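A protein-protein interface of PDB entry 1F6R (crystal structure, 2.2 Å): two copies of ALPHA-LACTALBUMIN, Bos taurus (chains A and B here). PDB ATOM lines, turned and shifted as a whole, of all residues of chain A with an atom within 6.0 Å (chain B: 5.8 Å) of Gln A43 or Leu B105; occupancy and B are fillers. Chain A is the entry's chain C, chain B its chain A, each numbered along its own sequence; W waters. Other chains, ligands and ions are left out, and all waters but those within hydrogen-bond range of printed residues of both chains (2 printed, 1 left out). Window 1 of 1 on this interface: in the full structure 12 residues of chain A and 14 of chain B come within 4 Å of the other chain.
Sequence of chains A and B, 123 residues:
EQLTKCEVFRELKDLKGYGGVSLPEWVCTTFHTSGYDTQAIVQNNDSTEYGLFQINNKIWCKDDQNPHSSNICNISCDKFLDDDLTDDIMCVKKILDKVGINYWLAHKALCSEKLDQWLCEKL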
ATOM      1  N   ILE A  41     -19.887  11.038   3.378  1.00  0.00           N
ATOM      2  CA  ILE A  41     -19.910   9.717   2.767  1.00  0.00           C
ATOM      3  C   ILE A  41     -18.841   8.881   3.443  1.00  0.00           C
ATOM      4  O   ILE A  41     -17.721   9.331   3.598  1.00  0.00           O
ATOM      5  CB  ILE A  41     -19.660   9.784   1.245  1.00  0.00           C
ATOM      6  CG1 ILE A  41     -19.705   8.377   0.650  1.00  0.00           C
ATOM      7  CG2 ILE A  41     -18.329  10.435   0.960  1.00  0.00           C
ATOM      8  CD1 ILE A  41     -19.609   8.353  -0.865  1.00  0.00           C
ATOM      9  N   VAL A  42     -19.212   7.690   3.895  1.00  0.00           N
ATOM     10  CA  VAL A  42     -18.271   6.788   4.552  1.00  0.00           C
ATOM     11  C   VAL A  42     -18.365   5.416   3.908  1.00  0.00           C
ATOM     12  O   VAL A  42     -19.412   4.765   3.963  1.00  0.00           O
ATOM     13  CB  VAL A  42     -18.571   6.610   6.045  1.00  0.00           C
ATOM     14  CG1 VAL A  42     -17.457   5.828   6.695  1.00  0.00           C
ATOM     15  CG2 VAL A  42     -18.704   7.930   6.695  1.00  0.00           C
ATOM     16  N   GLN A  43     -17.264   4.984   3.299  1.00  0.00           N
ATOM     17  CA  GLN A  43     -17.204   3.695   2.628  1.00  0.00           C
ATOM     18  C   GLN A  43     -16.475   2.696   3.513  1.00  0.00           C
ATOM     19  O   GLN A  43     -15.381   2.965   3.983  1.00  0.00           O
ATOM     20  CB  GLN A  43     -16.471   3.842   1.290  1.00  0.00           C
ATOM     21  CG  GLN A  43     -16.528   2.617   0.412  1.00  0.00           C
ATOM     22  CD  GLN A  43     -15.953   2.855  -0.974  1.00  0.00           C
ATOM     23  OE1 GLN A  43     -15.982   3.967  -1.479  1.00  0.00           O
ATOM     24  NE2 GLN A  43     -15.425   1.800  -1.592  1.00  0.00           N
ATOM     25  N   ASN A  44     -17.103   1.557   3.770  1.00  0.00           N
ATOM     26  CA  ASN A  44     -16.492   0.510   4.572  1.00  0.00           C
ATOM     27  C   ASN A  44     -16.304  -0.629   3.586  1.00  0.00           C
ATOM     28  O   ASN A  44     -16.629  -0.501   2.408  1.00  0.00           O
ATOM     29  CB  ASN A  44     -17.411   0.100   5.737  1.00  0.00           C
ATOM     30  CG  ASN A  44     -17.472   1.175   6.841  1.00  0.00           C
ATOM     31  OD1 ASN A  44     -18.540   1.715   7.148  1.00  0.00           O
ATOM     32  ND2 ASN A  44     -16.320   1.491   7.429  1.00  0.00           N
ATOM     33  N   ASN A  45     -15.777  -1.746   4.044  1.00  0.00           N
ATOM     34  CA  ASN A  45     -15.567  -2.841   3.121  1.00  0.00           C
ATOM     35  C   ASN A  45     -16.870  -3.416   2.557  1.00  0.00           C
ATOM     36  O   ASN A  45     -16.924  -3.832   1.406  1.00  0.00           O
ATOM     37  CB  ASN A  45     -14.755  -3.943   3.799  1.00  0.00           C
ATOM     38  CG  ASN A  45     -14.710  -5.203   2.979  1.00  0.00           C
ATOM     39  OD1 ASN A  45     -15.055  -6.281   3.467  1.00  0.00           O
ATOM     40  ND2 ASN A  45     -14.298  -5.078   1.715  1.00  0.00           N
ATOM     41  N   SER A  47     -20.235  -1.827   3.061  1.00  0.00           N
ATOM     42  CA  SER A  47     -21.270  -0.848   2.787  1.00  0.00           C
ATOM     43  C   SER A  47     -20.744   0.578   2.812  1.00  0.00           C
ATOM     44  O   SER A  47     -19.610   0.838   3.213  1.00  0.00           O
ATOM     45  CB  SER A  47     -22.401  -0.999   3.804  1.00  0.00           C
ATOM     46  OG  SER A  47     -21.904  -0.911   5.128  1.00  0.00           O
ATOM     47  N   THR A  48     -21.584   1.502   2.374  1.00  0.00           N
ATOM     48  CA  THR A  48     -21.234   2.904   2.361  1.00  0.00           C
ATOM     49  C   THR A  48     -22.467   3.671   2.848  1.00  0.00           C
ATOM     50  O   THR A  48     -23.601   3.344   2.476  1.00  0.00           O
ATOM     51  CB  THR A  48     -20.843   3.314   0.938  1.00  0.00           C
ATOM     52  OG1 THR A  48     -19.750   2.495   0.517  1.00  0.00           O
ATOM     53  CG2 THR A  48     -20.438   4.767   0.874  1.00  0.00           C
ATOM     54  N   GLU A  49     -22.255   4.666   3.702  1.00  0.00           N
ATOM     55  CA  GLU A  49     -23.362   5.458   4.221  1.00  0.00           C
ATOM     56  C   GLU A  49     -23.301   6.839   3.620  1.00  0.00           C
ATOM     57  O   GLU A  49     -22.232   7.438   3.494  1.00  0.00           O
ATOM     58  CB  GLU A  49     -23.316   5.458   5.734  1.00  0.00           C
ATOM     59  CG  GLU A  49     -23.409   4.024   6.193  1.00  0.00           C
ATOM     60  CD  GLU A  49     -23.325   3.885   7.666  1.00  0.00           C
ATOM     61  OE1 GLU A  49     -22.595   4.693   8.281  1.00  0.00           O
ATOM     62  OE2 GLU A  49     -23.986   2.968   8.207  1.00  0.00           O
ATOM     63  N   TYR A  50     -24.472   7.321   3.232  1.00  0.00           N
ATOM     64  CA  TYR A  50     -24.602   8.580   2.535  1.00  0.00           C
ATOM     65  C   TYR A  50     -25.365   9.722   3.176  1.00  0.00           C
ATOM     66  O   TYR A  50     -26.461   9.526   3.705  1.00  0.00           O
ATOM     67  CB  TYR A  50     -25.279   8.329   1.183  1.00  0.00           C
ATOM     68  CG  TYR A  50     -24.492   7.504   0.187  1.00  0.00           C
ATOM     69  CD1 TYR A  50     -23.866   8.111  -0.916  1.00  0.00           C
ATOM     70  CD2 TYR A  50     -24.423   6.111   0.305  1.00  0.00           C
ATOM     71  CE1 TYR A  50     -23.204   7.352  -1.876  1.00  0.00           C
ATOM     72  CE2 TYR A  50     -23.762   5.347  -0.650  1.00  0.00           C
ATOM     73  CZ  TYR A  50     -23.162   5.971  -1.739  1.00  0.00           C
ATOM     74  OH  TYR A  50     -22.560   5.200  -2.707  1.00  0.00           O
ATOM     75  N   ASN A  57     -26.224   1.849   1.791  1.00  0.00           N
ATOM     76  CA  ASN A  57     -26.509   1.179   0.537  1.00  0.00           C
ATOM     77  C   ASN A  57     -26.797  -0.329   0.611  1.00  0.00           C
ATOM     78  O   ASN A  57     -26.881  -0.987  -0.418  1.00  0.00           O
ATOM     79  CB  ASN A  57     -25.335   1.409  -0.410  1.00  0.00           C
ATOM     80  CG  ASN A  57     -24.051   0.739   0.079  1.00  0.00           C
ATOM     81  OD1 ASN A  57     -24.001   0.174   1.182  1.00  0.00           O
ATOM     82  ND2 ASN A  57     -23.015   0.797  -0.736  1.00  0.00           N
ATOM     83  N   ASP A  63     -26.414   1.210  -5.171  1.00  0.00           N
ATOM     84  CA  ASP A  63     -25.002   1.556  -5.354  1.00  0.00           C
ATOM     85  C   ASP A  63     -24.315   0.704  -6.408  1.00  0.00           C
ATOM     86  O   ASP A  63     -24.862  -0.297  -6.866  1.00  0.00           O
ATOM     87  CB  ASP A  63     -24.247   1.249  -4.060  1.00  0.00           C
ATOM     88  CG  ASP A  63     -23.613   2.419  -3.518  1.00  0.00           C
ATOM     89  OD1 ASP A  63     -23.783   3.465  -4.157  1.00  0.00           O
ATOM     90  OD2 ASP A  63     -22.959   2.317  -2.481  1.00  0.00           O
ATOM     91  N   ASP A  64     -23.077   1.084  -6.722  1.00  0.00           N
ATOM     92  CA  ASP A  64     -22.215   0.343  -7.637  1.00  0.00           C
ATOM     93  C   ASP A  64     -21.686  -0.786  -6.738  1.00  0.00           C
ATOM     94  O   ASP A  64     -21.424  -1.899  -7.173  1.00  0.00           O
ATOM     95  CB  ASP A  64     -21.032   1.213  -8.069  1.00  0.00           C
ATOM     96  CG  ASP A  64     -21.175   1.753  -9.480  1.00  0.00           C
ATOM     97  OD1 ASP A  64     -22.269   1.615 -10.075  1.00  0.00           O
ATOM     98  OD2 ASP A  64     -20.176   2.318  -9.989  1.00  0.00           O
ATOM     99  N   GLN A  65     -21.530  -0.463  -5.464  1.00  0.00           N
ATOM    100  CA  GLN A  65     -21.056  -1.417  -4.497  1.00  0.00           C
ATOM    101  C   GLN A  65     -22.097  -2.518  -4.238  1.00  0.00           C
ATOM    102  O   GLN A  65     -21.761  -3.699  -4.259  1.00  0.00           O
ATOM    103  CB  GLN A  65     -20.715  -0.693  -3.206  1.00  0.00           C
ATOM    104  CG  GLN A  65     -20.052  -1.562  -2.199  1.00  0.00           C
ATOM    105  CD  GLN A  65     -19.669  -0.803  -0.971  1.00  0.00           C
ATOM    106  OE1 GLN A  65     -18.565  -0.952  -0.456  1.00  0.00           O
ATOM    107  NE2 GLN A  65     -20.572   0.027  -0.487  1.00  0.00           N
ATOM    108  N   GLU B  49      -9.378   0.852   7.561  1.00  0.00           N
ATOM    109  CA  GLU B  49      -8.956   1.548   6.351  1.00  0.00           C
ATOM    110  C   GLU B  49      -7.799   2.480   6.651  1.00  0.00           C
ATOM    111  O   GLU B  49      -7.806   3.166   7.666  1.00  0.00           O
ATOM    112  CB  GLU B  49     -10.104   2.320   5.753  1.00  0.00           C
ATOM    113  CG  GLU B  49     -10.929   1.463   4.875  1.00  0.00           C
ATOM    114  CD  GLU B  49     -12.283   1.317   5.434  1.00  0.00           C
ATOM    115  OE1 GLU B  49     -12.514   0.346   6.194  1.00  0.00           O
ATOM    116  OE2 GLU B  49     -13.112   2.195   5.128  1.00  0.00           O
ATOM    117  N   ILE B 101     -11.565   3.140 -11.125  1.00  0.00           N
ATOM    118  CA  ILE B 101     -11.701   4.311 -10.262  1.00  0.00           C
ATOM    119  C   ILE B 101     -12.976   4.364  -9.395  1.00  0.00           C
ATOM    120  O   ILE B 101     -12.944   4.877  -8.272  1.00  0.00           O
ATOM    121  CB  ILE B 101     -11.578   5.633 -11.097  1.00  0.00           C
ATOM    122  CG1 ILE B 101     -11.505   6.836 -10.154  1.00  0.00           C
ATOM    123  CG2 ILE B 101     -12.750   5.780 -12.066  1.00  0.00           C
ATOM    124  CD1 ILE B 101     -10.393   6.751  -9.157  1.00  0.00           C
ATOM    125  N   ASN B 102     -14.079   3.813  -9.896  1.00  0.00           N
ATOM    126  CA  ASN B 102     -15.326   3.849  -9.144  1.00  0.00           C
ATOM    127  C   ASN B 102     -15.395   2.807  -8.048  1.00  0.00           C
ATOM    128  O   ASN B 102     -16.452   2.476  -7.526  1.00  0.00           O
ATOM    129  CB  ASN B 102     -16.535   3.765 -10.078  1.00  0.00           C
ATOM    130  CG  ASN B 102     -16.758   5.067 -10.837  1.00  0.00           C
ATOM    131  OD1 ASN B 102     -16.441   6.151 -10.342  1.00  0.00           O
ATOM    132  ND2 ASN B 102     -17.286   4.967 -12.038  1.00  0.00           N
ATOM    133  N   TYR B 103     -14.234   2.284  -7.712  1.00  0.00           N
ATOM    134  CA  TYR B 103     -14.140   1.380  -6.602  1.00  0.00           C
ATOM    135  C   TYR B 103     -14.358   2.334  -5.411  1.00  0.00           C
ATOM    136  O   TYR B 103     -14.883   1.945  -4.373  1.00  0.00           O
ATOM    137  CB  TYR B 103     -12.749   0.780  -6.559  1.00  0.00           C
ATOM    138  CG  TYR B 103     -12.449   0.093  -5.267  1.00  0.00           C
ATOM    139  CD1 TYR B 103     -13.060  -1.117  -4.954  1.00  0.00           C
ATOM    140  CD2 TYR B 103     -11.552   0.648  -4.351  1.00  0.00           C
ATOM    141  CE1 TYR B 103     -12.786  -1.765  -3.760  1.00  0.00           C
ATOM    142  CE2 TYR B 103     -11.269   0.012  -3.146  1.00  0.00           C
ATOM    143  CZ  TYR B 103     -11.890  -1.199  -2.858  1.00  0.00           C
ATOM    144  OH  TYR B 103     -11.608  -1.876  -1.691  1.00  0.00           O
ATOM    145  N   TRP B 104     -13.932   3.587  -5.583  1.00  0.00           N
ATOM    146  CA  TRP B 104     -14.112   4.653  -4.585  1.00  0.00           C
ATOM    147  C   TRP B 104     -15.454   5.285  -4.945  1.00  0.00           C
ATOM    148  O   TRP B 104     -15.567   6.052  -5.912  1.00  0.00           O
ATOM    149  CB  TRP B 104     -13.009   5.705  -4.705  1.00  0.00           C
ATOM    150  CG  TRP B 104     -11.719   5.258  -4.130  1.00  0.00           C
ATOM    151  CD1 TRP B 104     -11.289   5.428  -2.841  1.00  0.00           C
ATOM    152  CD2 TRP B 104     -10.669   4.567  -4.814  1.00  0.00           C
ATOM    153  NE1 TRP B 104     -10.030   4.887  -2.677  1.00  0.00           N
ATOM    154  CE2 TRP B 104      -9.621   4.353  -3.872  1.00  0.00           C
ATOM    155  CE3 TRP B 104     -10.506   4.110  -6.124  1.00  0.00           C
ATOM    156  CZ2 TRP B 104      -8.418   3.694  -4.209  1.00  0.00           C
ATOM    157  CZ3 TRP B 104      -9.307   3.451  -6.462  1.00  0.00           C
ATOM    158  CH2 TRP B 104      -8.282   3.254  -5.505  1.00  0.00           C
ATOM    159  N   LEU B 105     -16.479   4.939  -4.177  1.00  0.00           N
ATOM    160  CA  LEU B 105     -17.817   5.431  -4.443  1.00  0.00           C
ATOM    161  C   LEU B 105     -17.902   6.948  -4.506  1.00  0.00           C
ATOM    162  O   LEU B 105     -18.719   7.498  -5.232  1.00  0.00           O
ATOM    163  CB  LEU B 105     -18.790   4.859  -3.401  1.00  0.00           C
ATOM    164  CG  LEU B 105     -18.997   3.354  -3.618  1.00  0.00           C
ATOM    165  CD1 LEU B 105     -19.710   2.768  -2.443  1.00  0.00           C
ATOM    166  CD2 LEU B 105     -19.816   3.106  -4.888  1.00  0.00           C
ATOM    167  N   ALA B 106     -17.051   7.637  -3.766  1.00  0.00           N
ATOM    168  CA  ALA B 106     -17.094   9.090  -3.798  1.00  0.00           C
ATOM    169  C   ALA B 106     -16.749   9.599  -5.181  1.00  0.00           C
ATOM    170  O   ALA B 106     -17.224  10.658  -5.560  1.00  0.00           O
ATOM    171  CB  ALA B 106     -16.130   9.690  -2.773  1.00  0.00           C
ATOM    172  N   HIS B 107     -15.928   8.865  -5.941  1.00  0.00           N
ATOM    173  CA  HIS B 107     -15.569   9.338  -7.277  1.00  0.00           C
ATOM    174  C   HIS B 107     -16.784   9.390  -8.179  1.00  0.00           C
ATOM    175  O   HIS B 107     -17.053  10.397  -8.832  1.00  0.00           O
ATOM    176  CB  HIS B 107     -14.540   8.452  -7.972  1.00  0.00           C
ATOM    177  CG  HIS B 107     -14.312   8.837  -9.406  1.00  0.00           C
ATOM    178  ND1 HIS B 107     -15.019   8.280 -10.453  1.00  0.00           N
ATOM    179  CD2 HIS B 107     -13.513   9.786  -9.957  1.00  0.00           C
ATOM    180  CE1 HIS B 107     -14.670   8.871 -11.584  1.00  0.00           C
ATOM    181  NE2 HIS B 107     -13.758   9.787 -11.311  1.00  0.00           N
ATOM    182  N   LYS B 108     -17.506   8.282  -8.229  1.00  0.00           N
ATOM    183  CA  LYS B 108     -18.678   8.210  -9.068  1.00  0.00           C
ATOM    184  C   LYS B 108     -19.718   9.217  -8.611  1.00  0.00           C
ATOM    185  O   LYS B 108     -20.377   9.839  -9.423  1.00  0.00           O
ATOM    186  CB  LYS B 108     -19.278   6.807  -9.020  1.00  0.00           C
ATOM    187  CG  LYS B 108     -20.651   6.742  -9.633  1.00  0.00           C
ATOM    188  CD  LYS B 108     -20.577   6.276 -11.056  1.00  0.00           C
ATOM    189  CE  LYS B 108     -21.590   5.169 -11.322  1.00  0.00           C
ATOM    190  NZ  LYS B 108     -21.046   4.086 -12.199  1.00  0.00           N
ATOM    191  N   ALA B 109     -19.850   9.379  -7.300  1.00  0.00           N
ATOM    192  CA  ALA B 109     -20.836  10.282  -6.726  1.00  0.00           C
ATOM    193  C   ALA B 109     -20.520  11.774  -6.792  1.00  0.00           C
ATOM    194  O   ALA B 109     -21.376  12.564  -7.157  1.00  0.00           O
ATOM    195  CB  ALA B 109     -21.107   9.883  -5.264  1.00  0.00           C
ATOM    196  N   LEU B 110     -19.298  12.161  -6.448  1.00  0.00           N
ATOM    197  CA  LEU B 110     -18.939  13.576  -6.411  1.00  0.00           C
ATOM    198  C   LEU B 110     -17.761  14.063  -7.268  1.00  0.00           C
ATOM    199  O   LEU B 110     -17.479  15.264  -7.280  1.00  0.00           O
ATOM    200  CB  LEU B 110     -18.631  13.960  -4.961  1.00  0.00           C
ATOM    201  CG  LEU B 110     -19.593  13.598  -3.836  1.00  0.00           C
ATOM    202  CD1 LEU B 110     -18.849  13.471  -2.497  1.00  0.00           C
ATOM    203  CD2 LEU B 110     -20.610  14.692  -3.738  1.00  0.00           C
HETATM  204  O   HOH W   1     -15.332   6.487  -1.809  1.00  0.00           O
HETATM  205  O   HOH W   2     -21.954   6.331  -5.236  1.00  0.00           O
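The backbone carbonyl oxygen (O) of Tyr B103 is in hydrogen-bond range of the side-chain amide nitrogen (NE2) of Gln A43, at 2.8 Å. The backbone NH of Leu B105 lies within hydrogen-bond range of the side-chain amide oxygen of Gln A43, 2.9 Å away. The side-chain carboxylate (OD2) of Asp A64 is in salt-bridge range of the side-chain amino group (NZ) of Lys B108. The side-chain carboxylate of Glu B49 lies close to the backbone carbonyl oxygen of Gln A43, 2.7 Å away.
The backbone carbonyl oxygen (O) of Asn A44 lies close to the side-chain amide oxygen (OE1) of Gln A65, 3.5 Å away. NE2 of Gln A65 sits close to ND2 of Asn A57 (2.6 Å). The side-chain hydroxyl (OG1) of Thr A48 is in hydrogen-bond range of the side-chain amide nitrogen (NE2) of Gln A65 (2.8 Å). The side-chain amide oxygen of Asn A57 is in hydrogen-bond range of the backbone NH of Thr A48. ND1 of His B107 is in hydrogen-bond range of OD1 of Asn B102, 2.6 Å away. The side-chain carboxylate of Asp A63 sits at hydrogen-bond distance from the side-chain hydroxyl of Tyr A50.
Gln A43 touches just these residues of chain B: Glu B49, Tyr B103, Trp B104 and Leu B105. Leu B105 touches six residues of chain A. Of the printed residues of chain B, Gln A65 touches Leu B105. Of the printed residues of chain B, Thr A48 touches Leu B105 (3.0 Å). Printed residues of chain A within 4 Å of Lys B108: Asp A64 (3.0 Å). Ser A47 touches none of the printed residues of chain B.
1 position is printed for both chains.
Along chain B the printed residues that touch a printed residue of chain A span positions 49 to 108. Of the 13 printed residues of chain A, 8 touch a printed residue of chain B. Printed residues of chain A that touch a printed residue of chain B: Ile A41, Gln A43, Asn A44, Thr A48, Tyr A50, Asp A63, Asp A64 and Gln A65. Among the printed residues, Asp or Glu carboxylates within 4 Å of a Lys or Arg side-chain nitrogen of the other chain: Asp A64 with Lys B108 (3.0 Å).
Among the printed residues, merely in contact across the chains: Ile A41 with Ala B106 (3.9 Å), Gln A43 with Trp B104 (3.7 Å), Asn A44 with Glu B49 (3.8 Å), Thr A48 with Leu B105 (3.0 Å), Tyr A50 with Leu B105 (3.8 Å), Asp A63 with Leu B105 (3.3 Å), Asp A64 with Asn B102 (3.9 Å), Asp A64 with Leu B105 (3.9 Å) and Gln A65 with Leu B105 (3.5 Å).
Water W1 lies within hydrogen-bond range of OE1 of Gln A43, N of Ala B106 and N of Leu B105. Water W2 bridges OH of Tyr A50 (2.8 Å) and O of Leu B105 (3.4 Å).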
